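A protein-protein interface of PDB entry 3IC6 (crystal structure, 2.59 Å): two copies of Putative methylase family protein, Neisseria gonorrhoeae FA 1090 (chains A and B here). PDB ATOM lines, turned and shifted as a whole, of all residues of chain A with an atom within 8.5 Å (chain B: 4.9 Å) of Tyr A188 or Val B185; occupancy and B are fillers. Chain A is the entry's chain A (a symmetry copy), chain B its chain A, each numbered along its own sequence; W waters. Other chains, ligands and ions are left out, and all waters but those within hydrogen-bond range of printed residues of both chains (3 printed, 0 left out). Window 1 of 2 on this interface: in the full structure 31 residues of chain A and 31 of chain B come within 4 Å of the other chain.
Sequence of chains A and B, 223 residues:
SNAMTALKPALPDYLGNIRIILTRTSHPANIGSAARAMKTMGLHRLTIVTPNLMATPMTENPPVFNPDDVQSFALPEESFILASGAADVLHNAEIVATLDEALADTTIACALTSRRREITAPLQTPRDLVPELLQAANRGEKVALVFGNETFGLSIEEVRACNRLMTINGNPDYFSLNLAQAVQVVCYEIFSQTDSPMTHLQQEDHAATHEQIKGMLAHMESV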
ATOM      1  N   ALA A  37      23.752  -4.969  14.555  1.00  0.00           N
ATOM      2  CA  ALA A  37      22.430  -4.354  14.655  1.00  0.00           C
ATOM      3  C   ALA A  37      22.512  -2.881  15.087  1.00  0.00           C
ATOM      4  O   ALA A  37      21.822  -2.026  14.530  1.00  0.00           O
ATOM      5  CB  ALA A  37      21.526  -5.165  15.593  1.00  0.00           C
ATOM      6  N   MET A  38      23.364  -2.589  16.065  1.00  0.00           N
ATOM      7  CA  MET A  38      23.475  -1.234  16.595  1.00  0.00           C
ATOM      8  C   MET A  38      23.998  -0.260  15.561  1.00  0.00           C
ATOM      9  O   MET A  38      23.382   0.774  15.326  1.00  0.00           O
ATOM     10  CB  MET A  38      24.397  -1.187  17.791  1.00  0.00           C
ATOM     11  CG  MET A  38      23.807  -1.784  19.013  1.00  0.00           C
ATOM     12  SD  MET A  38      25.179  -2.049  20.337  1.00  0.00           S
ATOM     13  CE  MET A  38      25.716  -0.195  20.623  1.00  0.00           C
ATOM     14  N   THR A  40      24.291  -0.297  12.315  1.00  0.00           N
ATOM     15  CA  THR A  40      23.339  -0.168  11.237  1.00  0.00           C
ATOM     16  C   THR A  40      22.246   0.846  11.562  1.00  0.00           C
ATOM     17  O   THR A  40      21.648   1.441  10.661  1.00  0.00           O
ATOM     18  CB  THR A  40      22.698  -1.532  10.982  1.00  0.00           C
ATOM     19  OG1 THR A  40      23.716  -2.426  10.553  1.00  0.00           O
ATOM     20  CG2 THR A  40      21.635  -1.475   9.926  1.00  0.00           C
ATOM     21  N   MET A  41      21.957   1.022  12.846  1.00  0.00           N
ATOM     22  CA  MET A  41      20.869   1.903  13.240  1.00  0.00           C
ATOM     23  C   MET A  41      21.466   3.121  13.898  1.00  0.00           C
ATOM     24  O   MET A  41      20.768   3.877  14.554  1.00  0.00           O
ATOM     25  CB  MET A  41      19.858   1.195  14.140  1.00  0.00           C
ATOM     26  CG  MET A  41      19.031   0.156  13.416  1.00  0.00           C
ATOM     27  SD  MET A  41      18.101   0.937  11.903  1.00  0.00           S
ATOM     28  CE  MET A  41      17.381  -0.656  11.055  1.00  0.00           C
ATOM     29  N   GLY A  42      22.765   3.309  13.693  1.00  0.00           N
ATOM     30  CA  GLY A  42      23.461   4.496  14.162  1.00  0.00           C
ATOM     31  C   GLY A  42      23.757   4.608  15.648  1.00  0.00           C
ATOM     32  O   GLY A  42      23.956   5.709  16.161  1.00  0.00           O
ATOM     33  N   LEU A  43      23.818   3.480  16.348  1.00  0.00           N
ATOM     34  CA  LEU A  43      24.175   3.479  17.777  1.00  0.00           C
ATOM     35  C   LEU A  43      25.576   2.887  17.910  1.00  0.00           C
ATOM     36  O   LEU A  43      25.887   1.888  17.248  1.00  0.00           O
ATOM     37  CB  LEU A  43      23.163   2.673  18.574  1.00  0.00           C
ATOM     38  CG  LEU A  43      21.717   3.177  18.540  1.00  0.00           C
ATOM     39  CD1 LEU A  43      20.758   2.051  18.792  1.00  0.00           C
ATOM     40  CD2 LEU A  43      21.469   4.314  19.524  1.00  0.00           C
ATOM     41  N   PRO A 126       8.496  -0.472  22.857  1.00  0.00           N
ATOM     42  CA  PRO A 126       9.494   0.459  22.320  1.00  0.00           C
ATOM     43  C   PRO A 126       8.864   1.636  21.554  1.00  0.00           C
ATOM     44  O   PRO A 126       9.299   2.772  21.741  1.00  0.00           O
ATOM     45  CB  PRO A 126      10.334  -0.427  21.400  1.00  0.00           C
ATOM     46  CG  PRO A 126      10.144  -1.805  21.957  1.00  0.00           C
ATOM     47  CD  PRO A 126       8.720  -1.842  22.361  1.00  0.00           C
ATOM     48  N   ARG A 127       7.829   1.382  20.744  1.00  0.00           N
ATOM     49  CA  ARG A 127       7.046   2.482  20.143  1.00  0.00           C
ATOM     50  C   ARG A 127       6.755   3.594  21.160  1.00  0.00           C
ATOM     51  O   ARG A 127       7.011   4.758  20.892  1.00  0.00           O
ATOM     52  CB  ARG A 127       5.740   1.984  19.517  1.00  0.00           C
ATOM     53  CG  ARG A 127       4.910   3.055  18.780  1.00  0.00           C
ATOM     54  CD  ARG A 127       5.561   3.629  17.478  1.00  0.00           C
ATOM     55  NE  ARG A 127       6.387   2.615  16.828  1.00  0.00           N
ATOM     56  CZ  ARG A 127       5.929   1.664  16.015  1.00  0.00           C
ATOM     57  NH1 ARG A 127       6.763   0.760  15.548  1.00  0.00           N
ATOM     58  NH2 ARG A 127       4.648   1.611  15.668  1.00  0.00           N
ATOM     59  N   VAL A 130      10.379   5.004  23.323  1.00  0.00           N
ATOM     60  CA  VAL A 130      11.444   5.699  22.568  1.00  0.00           C
ATOM     61  C   VAL A 130      11.350   7.260  22.537  1.00  0.00           C
ATOM     62  O   VAL A 130      12.381   7.926  22.711  1.00  0.00           O
ATOM     63  CB  VAL A 130      11.661   5.059  21.146  1.00  0.00           C
ATOM     64  CG1 VAL A 130      12.435   5.984  20.207  1.00  0.00           C
ATOM     65  CG2 VAL A 130      12.380   3.752  21.272  1.00  0.00           C
ATOM     66  N   LEU A 177      11.294 -14.779  19.953  1.00  0.00           N
ATOM     67  CA  LEU A 177      12.149 -13.728  19.464  1.00  0.00           C
ATOM     68  C   LEU A 177      13.480 -13.865  20.157  1.00  0.00           C
ATOM     69  O   LEU A 177      13.563 -13.665  21.367  1.00  0.00           O
ATOM     70  CB  LEU A 177      11.531 -12.366  19.818  1.00  0.00           C
ATOM     71  CG  LEU A 177      12.088 -11.136  19.088  1.00  0.00           C
ATOM     72  CD1 LEU A 177      11.341 -11.007  17.817  1.00  0.00           C
ATOM     73  CD2 LEU A 177      11.896  -9.870  19.901  1.00  0.00           C
ATOM     74  N   ALA A 180      19.310 -11.556  19.605  1.00  0.00           N
ATOM     75  CA  ALA A 180      19.756 -10.755  18.452  1.00  0.00           C
ATOM     76  C   ALA A 180      18.568 -10.076  17.759  1.00  0.00           C
ATOM     77  O   ALA A 180      18.668  -8.917  17.364  1.00  0.00           O
ATOM     78  CB  ALA A 180      20.533 -11.607  17.471  1.00  0.00           C
ATOM     79  N   GLN A 181      17.440 -10.774  17.627  1.00  0.00           N
ATOM     80  CA  GLN A 181      16.288 -10.187  16.968  1.00  0.00           C
ATOM     81  C   GLN A 181      15.708  -9.070  17.850  1.00  0.00           C
ATOM     82  O   GLN A 181      15.281  -8.020  17.338  1.00  0.00           O
ATOM     83  CB  GLN A 181      15.228 -11.238  16.627  1.00  0.00           C
ATOM     84  CG  GLN A 181      15.652 -12.323  15.631  1.00  0.00           C
ATOM     85  CD  GLN A 181      14.620 -13.505  15.561  1.00  0.00           C
ATOM     86  OE1 GLN A 181      14.306 -14.176  16.580  1.00  0.00           O
ATOM     87  NE2 GLN A 181      14.091 -13.761  14.334  1.00  0.00           N
ATOM     88  N   ALA A 182      15.724  -9.285  19.172  1.00  0.00           N
ATOM     89  CA  ALA A 182      15.256  -8.283  20.123  1.00  0.00           C
ATOM     90  C   ALA A 182      16.116  -7.049  20.096  1.00  0.00           C
ATOM     91  O   ALA A 182      15.593  -5.937  20.119  1.00  0.00           O
ATOM     92  CB  ALA A 182      15.203  -8.844  21.542  1.00  0.00           C
ATOM     93  N   VAL A 183      17.431  -7.206  20.057  1.00  0.00           N
ATOM     94  CA  VAL A 183      18.286  -6.019  19.986  1.00  0.00           C
ATOM     95  C   VAL A 183      17.986  -5.292  18.677  1.00  0.00           C
ATOM     96  O   VAL A 183      17.838  -4.082  18.653  1.00  0.00           O
ATOM     97  CB  VAL A 183      19.774  -6.387  20.060  1.00  0.00           C
ATOM     98  CG1 VAL A 183      20.642  -5.173  19.808  1.00  0.00           C
ATOM     99  CG2 VAL A 183      20.091  -6.962  21.401  1.00  0.00           C
ATOM    100  N   GLN A 184      17.860  -6.064  17.597  1.00  0.00           N
ATOM    101  CA  GLN A 184      17.535  -5.541  16.273  1.00  0.00           C
ATOM    102  C   GLN A 184      16.236  -4.755  16.272  1.00  0.00           C
ATOM    103  O   GLN A 184      16.170  -3.653  15.730  1.00  0.00           O
ATOM    104  CB  GLN A 184      17.416  -6.680  15.238  1.00  0.00           C
ATOM    105  CG  GLN A 184      17.128  -6.202  13.823  1.00  0.00           C
ATOM    106  CD  GLN A 184      18.247  -5.294  13.303  1.00  0.00           C
ATOM    107  OE1 GLN A 184      18.287  -4.082  13.569  1.00  0.00           O
ATOM    108  NE2 GLN A 184      19.177  -5.887  12.569  1.00  0.00           N
ATOM    109  N   VAL A 185      15.194  -5.332  16.850  1.00  0.00           N
ATOM    110  CA  VAL A 185      13.920  -4.646  16.885  1.00  0.00           C
ATOM    111  C   VAL A 185      14.017  -3.308  17.627  1.00  0.00           C
ATOM    112  O   VAL A 185      13.498  -2.302  17.153  1.00  0.00           O
ATOM    113  CB  VAL A 185      12.830  -5.528  17.492  1.00  0.00           C
ATOM    114  CG1 VAL A 185      11.637  -4.696  17.907  1.00  0.00           C
ATOM    115  CG2 VAL A 185      12.460  -6.598  16.508  1.00  0.00           C
ATOM    116  N   VAL A 186      14.696  -3.303  18.774  1.00  0.00           N
ATOM    117  CA  VAL A 186      14.829  -2.091  19.597  1.00  0.00           C
ATOM    118  C   VAL A 186      15.669  -0.996  18.931  1.00  0.00           C
ATOM    119  O   VAL A 186      15.327   0.183  18.996  1.00  0.00           O
ATOM    120  CB  VAL A 186      15.389  -2.441  21.003  1.00  0.00           C
ATOM    121  CG1 VAL A 186      15.830  -1.213  21.729  1.00  0.00           C
ATOM    122  CG2 VAL A 186      14.331  -3.178  21.815  1.00  0.00           C
ATOM    123  N   CYS A 187      16.768  -1.373  18.292  1.00  0.00           N
ATOM    124  CA  CYS A 187      17.573  -0.390  17.563  1.00  0.00           C
ATOM    125  C   CYS A 187      16.845   0.210  16.373  1.00  0.00           C
ATOM    126  O   CYS A 187      17.009   1.383  16.072  1.00  0.00           O
ATOM    127  CB  CYS A 187      18.795  -1.066  17.013  1.00  0.00           C
ATOM    128  SG  CYS A 187      19.910  -1.430  18.321  1.00  0.00           S
ATOM    129  N   TYR A 188      16.086  -0.631  15.673  1.00  0.00           N
ATOM    130  CA  TYR A 188      15.229  -0.184  14.619  1.00  0.00           C
ATOM    131  C   TYR A 188      14.219   0.847  15.129  1.00  0.00           C
ATOM    132  O   TYR A 188      14.039   1.909  14.505  1.00  0.00           O
ATOM    133  CB  TYR A 188      14.526  -1.367  13.941  1.00  0.00           C
ATOM    134  CG  TYR A 188      13.344  -0.935  13.131  1.00  0.00           C
ATOM    135  CD1 TYR A 188      13.511  -0.340  11.878  1.00  0.00           C
ATOM    136  CD2 TYR A 188      12.048  -1.065  13.634  1.00  0.00           C
ATOM    137  CE1 TYR A 188      12.411   0.088  11.131  1.00  0.00           C
ATOM    138  CE2 TYR A 188      10.943  -0.627  12.901  1.00  0.00           C
ATOM    139  CZ  TYR A 188      11.137  -0.054  11.652  1.00  0.00           C
ATOM    140  OH  TYR A 188      10.045   0.363  10.927  1.00  0.00           O
ATOM    141  N   GLU A 189      13.546   0.546  16.237  1.00  0.00           N
ATOM    142  CA  GLU A 189      12.561   1.481  16.753  1.00  0.00           C
ATOM    143  C   GLU A 189      13.196   2.829  17.032  1.00  0.00           C
ATOM    144  O   GLU A 189      12.657   3.860  16.622  1.00  0.00           O
ATOM    145  CB  GLU A 189      11.902   0.990  18.021  1.00  0.00           C
ATOM    146  CG  GLU A 189      10.777   1.900  18.458  1.00  0.00           C
ATOM    147  CD  GLU A 189       9.630   1.914  17.451  1.00  0.00           C
ATOM    148  OE1 GLU A 189       9.286   0.805  16.979  1.00  0.00           O
ATOM    149  OE2 GLU A 189       9.076   3.005  17.140  1.00  0.00           O
ATOM    150  N   ILE A 190      14.343   2.800  17.721  1.00  0.00           N
ATOM    151  CA  ILE A 190      15.071   4.016  18.074  1.00  0.00           C
ATOM    152  C   ILE A 190      15.321   4.827  16.824  1.00  0.00           C
ATOM    153  O   ILE A 190      14.922   5.992  16.742  1.00  0.00           O
ATOM    154  CB  ILE A 190      16.417   3.726  18.801  1.00  0.00           C
ATOM    155  CG1 ILE A 190      16.147   3.145  20.194  1.00  0.00           C
ATOM    156  CG2 ILE A 190      17.250   5.000  18.930  1.00  0.00           C
ATOM    157  CD1 ILE A 190      17.377   2.503  20.828  1.00  0.00           C
ATOM    158  N   PHE A 191      15.946   4.206  15.833  1.00  0.00           N
ATOM    159  CA  PHE A 191      16.269   4.930  14.620  1.00  0.00           C
ATOM    160  C   PHE A 191      15.036   5.380  13.897  1.00  0.00           C
ATOM    161  O   PHE A 191      15.023   6.469  13.331  1.00  0.00           O
ATOM    162  CB  PHE A 191      17.156   4.133  13.662  1.00  0.00           C
ATOM    163  CG  PHE A 191      17.687   4.972  12.540  1.00  0.00           C
ATOM    164  CD1 PHE A 191      18.877   5.697  12.697  1.00  0.00           C
ATOM    165  CD2 PHE A 191      16.956   5.107  11.337  1.00  0.00           C
ATOM    166  CE1 PHE A 191      19.350   6.532  11.639  1.00  0.00           C
ATOM    167  CE2 PHE A 191      17.402   5.944  10.298  1.00  0.00           C
ATOM    168  CZ  PHE A 191      18.607   6.655  10.450  1.00  0.00           C
ATOM    169  N   SER A 192      13.994   4.556  13.926  1.00  0.00           N
ATOM    170  CA  SER A 192      12.800   4.858  13.176  1.00  0.00           C
ATOM    171  C   SER A 192      12.155   6.151  13.670  1.00  0.00           C
ATOM    172  O   SER A 192      11.234   6.670  13.054  1.00  0.00           O
ATOM    173  CB  SER A 192      11.804   3.714  13.276  1.00  0.00           C
ATOM    174  OG  SER A 192      11.037   3.834  14.457  1.00  0.00           O
ATOM    175  N   GLN A 193      12.633   6.675  14.789  1.00  0.00           N
ATOM    176  CA  GLN A 193      11.990   7.843  15.337  1.00  0.00           C
ATOM    177  C   GLN A 193      12.869   9.087  15.261  1.00  0.00           C
ATOM    178  O   GLN A 193      12.491  10.119  15.777  1.00  0.00           O
ATOM    179  CB  GLN A 193      11.460   7.559  16.751  1.00  0.00           C
ATOM    180  CG  GLN A 193      10.224   6.625  16.734  1.00  0.00           C
ATOM    181  CD  GLN A 193       9.495   6.517  18.082  1.00  0.00           C
ATOM    182  OE1 GLN A 193       9.499   7.451  18.879  1.00  0.00           O
ATOM    183  NE2 GLN A 193       8.870   5.373  18.335  1.00  0.00           N
ATOM    184  N   THR A 194      14.016   9.004  14.592  1.00  0.00           N
ATOM    185  CA  THR A 194      14.953  10.125  14.580  1.00  0.00           C
ATOM    186  C   THR A 194      14.507  11.288  13.681  1.00  0.00           C
ATOM    187  O   THR A 194      15.112  12.367  13.700  1.00  0.00           O
ATOM    188  CB  THR A 194      16.425   9.706  14.284  1.00  0.00           C
ATOM    189  OG1 THR A 194      16.494   8.977  13.053  1.00  0.00           O
ATOM    190  CG2 THR A 194      16.989   8.831  15.404  1.00  0.00           C
ATOM    191  N   PRO B 126       8.740   1.260   6.251  1.00  0.00           N
ATOM    192  CA  PRO B 126       7.634   0.468   6.801  1.00  0.00           C
ATOM    193  C   PRO B 126       6.734   1.278   7.752  1.00  0.00           C
ATOM    194  O   PRO B 126       5.513   1.164   7.660  1.00  0.00           O
ATOM    195  CB  PRO B 126       8.351  -0.666   7.533  1.00  0.00           C
ATOM    196  CG  PRO B 126       9.675  -0.761   6.840  1.00  0.00           C
ATOM    197  CD  PRO B 126      10.044   0.647   6.563  1.00  0.00           C
ATOM    198  N   ARG B 127       7.319   2.116   8.616  1.00  0.00           N
ATOM    199  CA  ARG B 127       6.518   3.073   9.408  1.00  0.00           C
ATOM    200  C   ARG B 127       5.432   3.747   8.557  1.00  0.00           C
ATOM    201  O   ARG B 127       4.271   3.759   8.935  1.00  0.00           O
ATOM    202  CB  ARG B 127       7.390   4.132  10.086  1.00  0.00           C
ATOM    203  CG  ARG B 127       6.642   5.111  11.014  1.00  0.00           C
ATOM    204  CD  ARG B 127       6.038   4.476  12.310  1.00  0.00           C
ATOM    205  NE  ARG B 127       6.857   3.355  12.762  1.00  0.00           N
ATOM    206  CZ  ARG B 127       7.962   3.465  13.497  1.00  0.00           C
ATOM    207  NH1 ARG B 127       8.657   2.384  13.779  1.00  0.00           N
ATOM    208  NH2 ARG B 127       8.377   4.643  13.949  1.00  0.00           N
ATOM    209  N   ILE B 168      14.207   0.285   4.379  1.00  0.00           N
ATOM    210  CA  ILE B 168      14.487   0.353   5.793  1.00  0.00           C
ATOM    211  C   ILE B 168      15.668   1.290   5.969  1.00  0.00           C
ATOM    212  O   ILE B 168      16.766   0.990   5.510  1.00  0.00           O
ATOM    213  CB  ILE B 168      14.803  -1.051   6.365  1.00  0.00           C
ATOM    214  CG1 ILE B 168      13.566  -1.952   6.241  1.00  0.00           C
ATOM    215  CG2 ILE B 168      15.277  -0.966   7.826  1.00  0.00           C
ATOM    216  CD1 ILE B 168      13.805  -3.415   6.572  1.00  0.00           C
ATOM    217  N   LEU B 177      22.033  -5.321   7.214  1.00  0.00           N
ATOM    218  CA  LEU B 177      20.845  -5.938   7.743  1.00  0.00           C
ATOM    219  C   LEU B 177      20.570  -7.173   6.922  1.00  0.00           C
ATOM    220  O   LEU B 177      20.247  -7.063   5.741  1.00  0.00           O
ATOM    221  CB  LEU B 177      19.663  -4.965   7.606  1.00  0.00           C
ATOM    222  CG  LEU B 177      18.402  -5.281   8.421  1.00  0.00           C
ATOM    223  CD1 LEU B 177      18.585  -4.677   9.759  1.00  0.00           C
ATOM    224  CD2 LEU B 177      17.161  -4.687   7.781  1.00  0.00           C
ATOM    225  N   GLN B 181      16.797 -10.507   9.429  1.00  0.00           N
ATOM    226  CA  GLN B 181      16.591  -9.330  10.253  1.00  0.00           C
ATOM    227  C   GLN B 181      15.588  -8.393   9.562  1.00  0.00           C
ATOM    228  O   GLN B 181      14.734  -7.780  10.228  1.00  0.00           O
ATOM    229  CB  GLN B 181      17.906  -8.611  10.562  1.00  0.00           C
ATOM    230  CG  GLN B 181      18.928  -9.404  11.384  1.00  0.00           C
ATOM    231  CD  GLN B 181      20.339  -8.713  11.409  1.00  0.00           C
ATOM    232  OE1 GLN B 181      20.974  -8.459  10.350  1.00  0.00           O
ATOM    233  NE2 GLN B 181      20.831  -8.410  12.639  1.00  0.00           N
ATOM    234  N   ALA B 182      15.672  -8.308   8.228  1.00  0.00           N
ATOM    235  CA  ALA B 182      14.745  -7.498   7.445  1.00  0.00           C
ATOM    236  C   ALA B 182      13.337  -8.022   7.538  1.00  0.00           C
ATOM    237  O   ALA B 182      12.401  -7.240   7.691  1.00  0.00           O
ATOM    238  CB  ALA B 182      15.171  -7.422   5.981  1.00  0.00           C
ATOM    239  N   VAL B 183      13.151  -9.330   7.441  1.00  0.00           N
ATOM    240  CA  VAL B 183      11.794  -9.866   7.572  1.00  0.00           C
ATOM    241  C   VAL B 183      11.290  -9.549   8.979  1.00  0.00           C
ATOM    242  O   VAL B 183      10.167  -9.109   9.155  1.00  0.00           O
ATOM    243  CB  VAL B 183      11.756 -11.380   7.323  1.00  0.00           C
ATOM    244  CG1 VAL B 183      10.386 -11.943   7.635  1.00  0.00           C
ATOM    245  CG2 VAL B 183      12.107 -11.673   5.901  1.00  0.00           C
ATOM    246  N   GLN B 184      12.162  -9.745   9.968  1.00  0.00           N
ATOM    247  CA  GLN B 184      11.861  -9.455  11.368  1.00  0.00           C
ATOM    248  C   GLN B 184      11.442  -8.012  11.576  1.00  0.00           C
ATOM    249  O   GLN B 184      10.448  -7.738  12.246  1.00  0.00           O
ATOM    250  CB  GLN B 184      13.079  -9.744  12.270  1.00  0.00           C
ATOM    251  CG  GLN B 184      12.821  -9.513  13.751  1.00  0.00           C
ATOM    252  CD  GLN B 184      11.705 -10.424  14.271  1.00  0.00           C
ATOM    253  OE1 GLN B 184      10.504 -10.131  14.145  1.00  0.00           O
ATOM    254  NE2 GLN B 184      12.100 -11.550  14.845  1.00  0.00           N
ATOM    255  N   VAL B 185      12.215  -7.086  11.031  1.00  0.00           N
ATOM    256  CA  VAL B 185      11.882  -5.686  11.189  1.00  0.00           C
ATOM    257  C   VAL B 185      10.504  -5.362  10.602  1.00  0.00           C
ATOM    258  O   VAL B 185       9.713  -4.667  11.235  1.00  0.00           O
ATOM    259  CB  VAL B 185      12.959  -4.787  10.584  1.00  0.00           C
ATOM    260  CG1 VAL B 185      12.431  -3.384  10.377  1.00  0.00           C
ATOM    261  CG2 VAL B 185      14.172  -4.811  11.466  1.00  0.00           C
ATOM    262  N   VAL B 186      10.221  -5.880   9.407  1.00  0.00           N
ATOM    263  CA  VAL B 186       8.948  -5.611   8.722  1.00  0.00           C
ATOM    264  C   VAL B 186       7.736  -6.225   9.433  1.00  0.00           C
ATOM    265  O   VAL B 186       6.685  -5.595   9.536  1.00  0.00           O
ATOM    266  CB  VAL B 186       9.014  -6.074   7.241  1.00  0.00           C
ATOM    267  CG1 VAL B 186       7.653  -6.109   6.625  1.00  0.00           C
ATOM    268  CG2 VAL B 186       9.924  -5.145   6.447  1.00  0.00           C
ATOM    269  N   CYS B 187       7.871  -7.449   9.923  1.00  0.00           N
ATOM    270  CA  CYS B 187       6.782  -8.064  10.686  1.00  0.00           C
ATOM    271  C   CYS B 187       6.500  -7.353  11.998  1.00  0.00           C
ATOM    272  O   CYS B 187       5.356  -7.254  12.417  1.00  0.00           O
ATOM    273  CB  CYS B 187       7.165  -9.470  11.042  1.00  0.00           C
ATOM    274  SG  CYS B 187       7.108 -10.482   9.607  1.00  0.00           S
ATOM    275  N   TYR B 188       7.569  -6.913  12.661  1.00  0.00           N
ATOM    276  CA  TYR B 188       7.455  -6.100  13.832  1.00  0.00           C
ATOM    277  C   TYR B 188       6.679  -4.813  13.538  1.00  0.00           C
ATOM    278  O   TYR B 188       5.761  -4.449  14.294  1.00  0.00           O
ATOM    279  CB  TYR B 188       8.835  -5.797  14.428  1.00  0.00           C
ATOM    280  CG  TYR B 188       8.798  -4.647  15.385  1.00  0.00           C
ATOM    281  CD1 TYR B 188       8.295  -4.804  16.679  1.00  0.00           C
ATOM    282  CD2 TYR B 188       9.214  -3.374  14.989  1.00  0.00           C
ATOM    283  CE1 TYR B 188       8.235  -3.727  17.566  1.00  0.00           C
ATOM    284  CE2 TYR B 188       9.145  -2.288  15.863  1.00  0.00           C
ATOM    285  CZ  TYR B 188       8.655  -2.477  17.148  1.00  0.00           C
ATOM    286  OH  TYR B 188       8.602  -1.408  18.010  1.00  0.00           O
ATOM    287  N   GLU B 189       7.044  -4.113  12.466  1.00  0.00           N
ATOM    288  CA  GLU B 189       6.354  -2.873  12.153  1.00  0.00           C
ATOM    289  C   GLU B 189       4.868  -3.117  11.976  1.00  0.00           C
ATOM    290  O   GLU B 189       4.052  -2.390  12.549  1.00  0.00           O
ATOM    291  CB  GLU B 189       6.884  -2.214  10.900  1.00  0.00           C
ATOM    292  CG  GLU B 189       6.261  -0.856  10.674  1.00  0.00           C
ATOM    293  CD  GLU B 189       6.635   0.134  11.774  1.00  0.00           C
ATOM    294  OE1 GLU B 189       7.833   0.136  12.144  1.00  0.00           O
ATOM    295  OE2 GLU B 189       5.757   0.902  12.258  1.00  0.00           O
HETATM  296  O   HOH W   1       6.318  -1.237  19.800  1.00  0.00           O
HETATM  297  O   HOH W   2      10.313   2.809   9.381  1.00  0.00           O
HETATM  298  O   HOH W   3      23.258  -8.078  13.623  1.00  0.00           O
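Of the printed residues of chain B, Arg A127 touches Arg B127, Tyr B188 and Glu B189.
Tyr A188 touches just these residues of chain B: Pro B126 (3.9 Å), Arg B127 (3.8 Å), Val B185 (3.6 Å), Tyr B188 (3.8 Å) and Glu B189 (2.5 Å).
Val B183 touches none of the printed residues of chain A.
Of the printed residues of chain A, Gln B184 touches Leu A177 and Gln A181.
Val B185 touches one residue of chain A.
The nearest residue of chain B that does not touch Tyr A188 is Ile B168 (4.5 Å).
The nearest printed residue of chain B that does not touch Pro A126 is Arg B127 (7.8 Å).
Of the 13 printed residues of chain B, 9 touch a printed residue of chain A.
Printed residues of chain B that touch a printed residue of chain A: Pro B126, Arg B127, Ile B168, Leu B177, Gln B181, Gln B184, Val B185, Tyr B188 and Glu B189.
Hydrophobic or aromatic side chains of chain B within 4 Å of the printed part of chain A: Pro B126, Ile B168, Leu B177, Val B185 and Tyr B188.
Of the 25 printed residues of chain A, 11 touch a printed residue of chain B.
Among the printed residues, 19 pairs touch across the chains.
CG2 of Ile B168 touches CE of Met A41 (3.9 Å).
CB of Pro A126 touches OH of Tyr B188, 3.9 Å away.
NH1 of Arg A127 touches OH of Tyr B188, 3.8 Å away.
Gln B184 touches Leu A177.
CD1 of Leu B177 touches NE2 of Gln A184 (3.1 Å).
Val A185 touches Tyr B188.
Tyr A188 touches Pro B126 (OH to CB, 3.9 Å).
Tyr A188 touches Arg B127.
Val B185 touches Tyr A188.
Tyr A188 touches Tyr B188 (CE2 to CE2, 3.8 Å).
O of Arg A127 lies within hydrogen-bond range of NE2 of Gln A193.
NE of Arg A127 is in salt-bridge range of OE2 of Glu A189 (2.7 Å).
The side-chain hydroxyl (OG) of Ser A192 sits at hydrogen-bond distance from the backbone carbonyl oxygen (O) of Glu A189.
The guanidinium group of Arg B127 is in salt-bridge range of the side-chain carboxylate of Glu B189.
NE2 of Gln A193 lies within hydrogen-bond range of OE2 of Glu A189 (2.7 Å).
Water W3 lies within hydrogen-bond range of the side-chain amide nitrogen (NE2) of Gln B181 (2.6 Å) and the backbone NH (N) of Ala A37 (3.3 Å).
Water W1 lies within hydrogen-bond range of OH of Tyr B188 (2.9 Å) and N of Arg A127 (3.2 Å).
Water W2 lies within hydrogen-bond range of the side-chain hydroxyl of Tyr A188 (2.9 Å) and the backbone NH of Arg B127 (3.2 Å).
Arg A127 touches Glu B189, and with the chains exchanged Glu A189 touches Arg B127.
Gln A181 touches Gln B184, and with the chains exchanged Gln A184 touches Gln B181.
Tyr B188 touches its own counterpart, Tyr A188.
Tyr A188 touches Glu B189, and with the chains exchanged Glu A189 touches Tyr B188.
NE2 of Gln B181 lies close to NE2 of Gln A184 (3.0 Å).
The side-chain amide nitrogen (NE2) of Gln B184 sits close to the side-chain amide nitrogen (NE2) of Gln A181 (3.0 Å).
The side-chain carboxylate of Glu A189 is in salt-bridge range of the guanidinium group of Arg B127 (3.4 Å).
The side-chain hydroxyl (OH) of Tyr B188 is in hydrogen-bond range of the side-chain carboxylate (OE1) of Glu A189 (2.5 Å).
The guanidinium group (NH1) of Arg A127 lies close to the guanidinium group (NH1) of Arg B127.
The side-chain carboxylate (OE2) of Glu B189 lies within salt-bridge range of the guanidinium group (NH1) of Arg A127 (3.4 Å).
OG of Ser A192 is in hydrogen-bond range of NH2 of Arg B127, at 2.8 Å.
OE1 of Glu B189 is in hydrogen-bond range of OH of Tyr A188 (2.5 Å).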
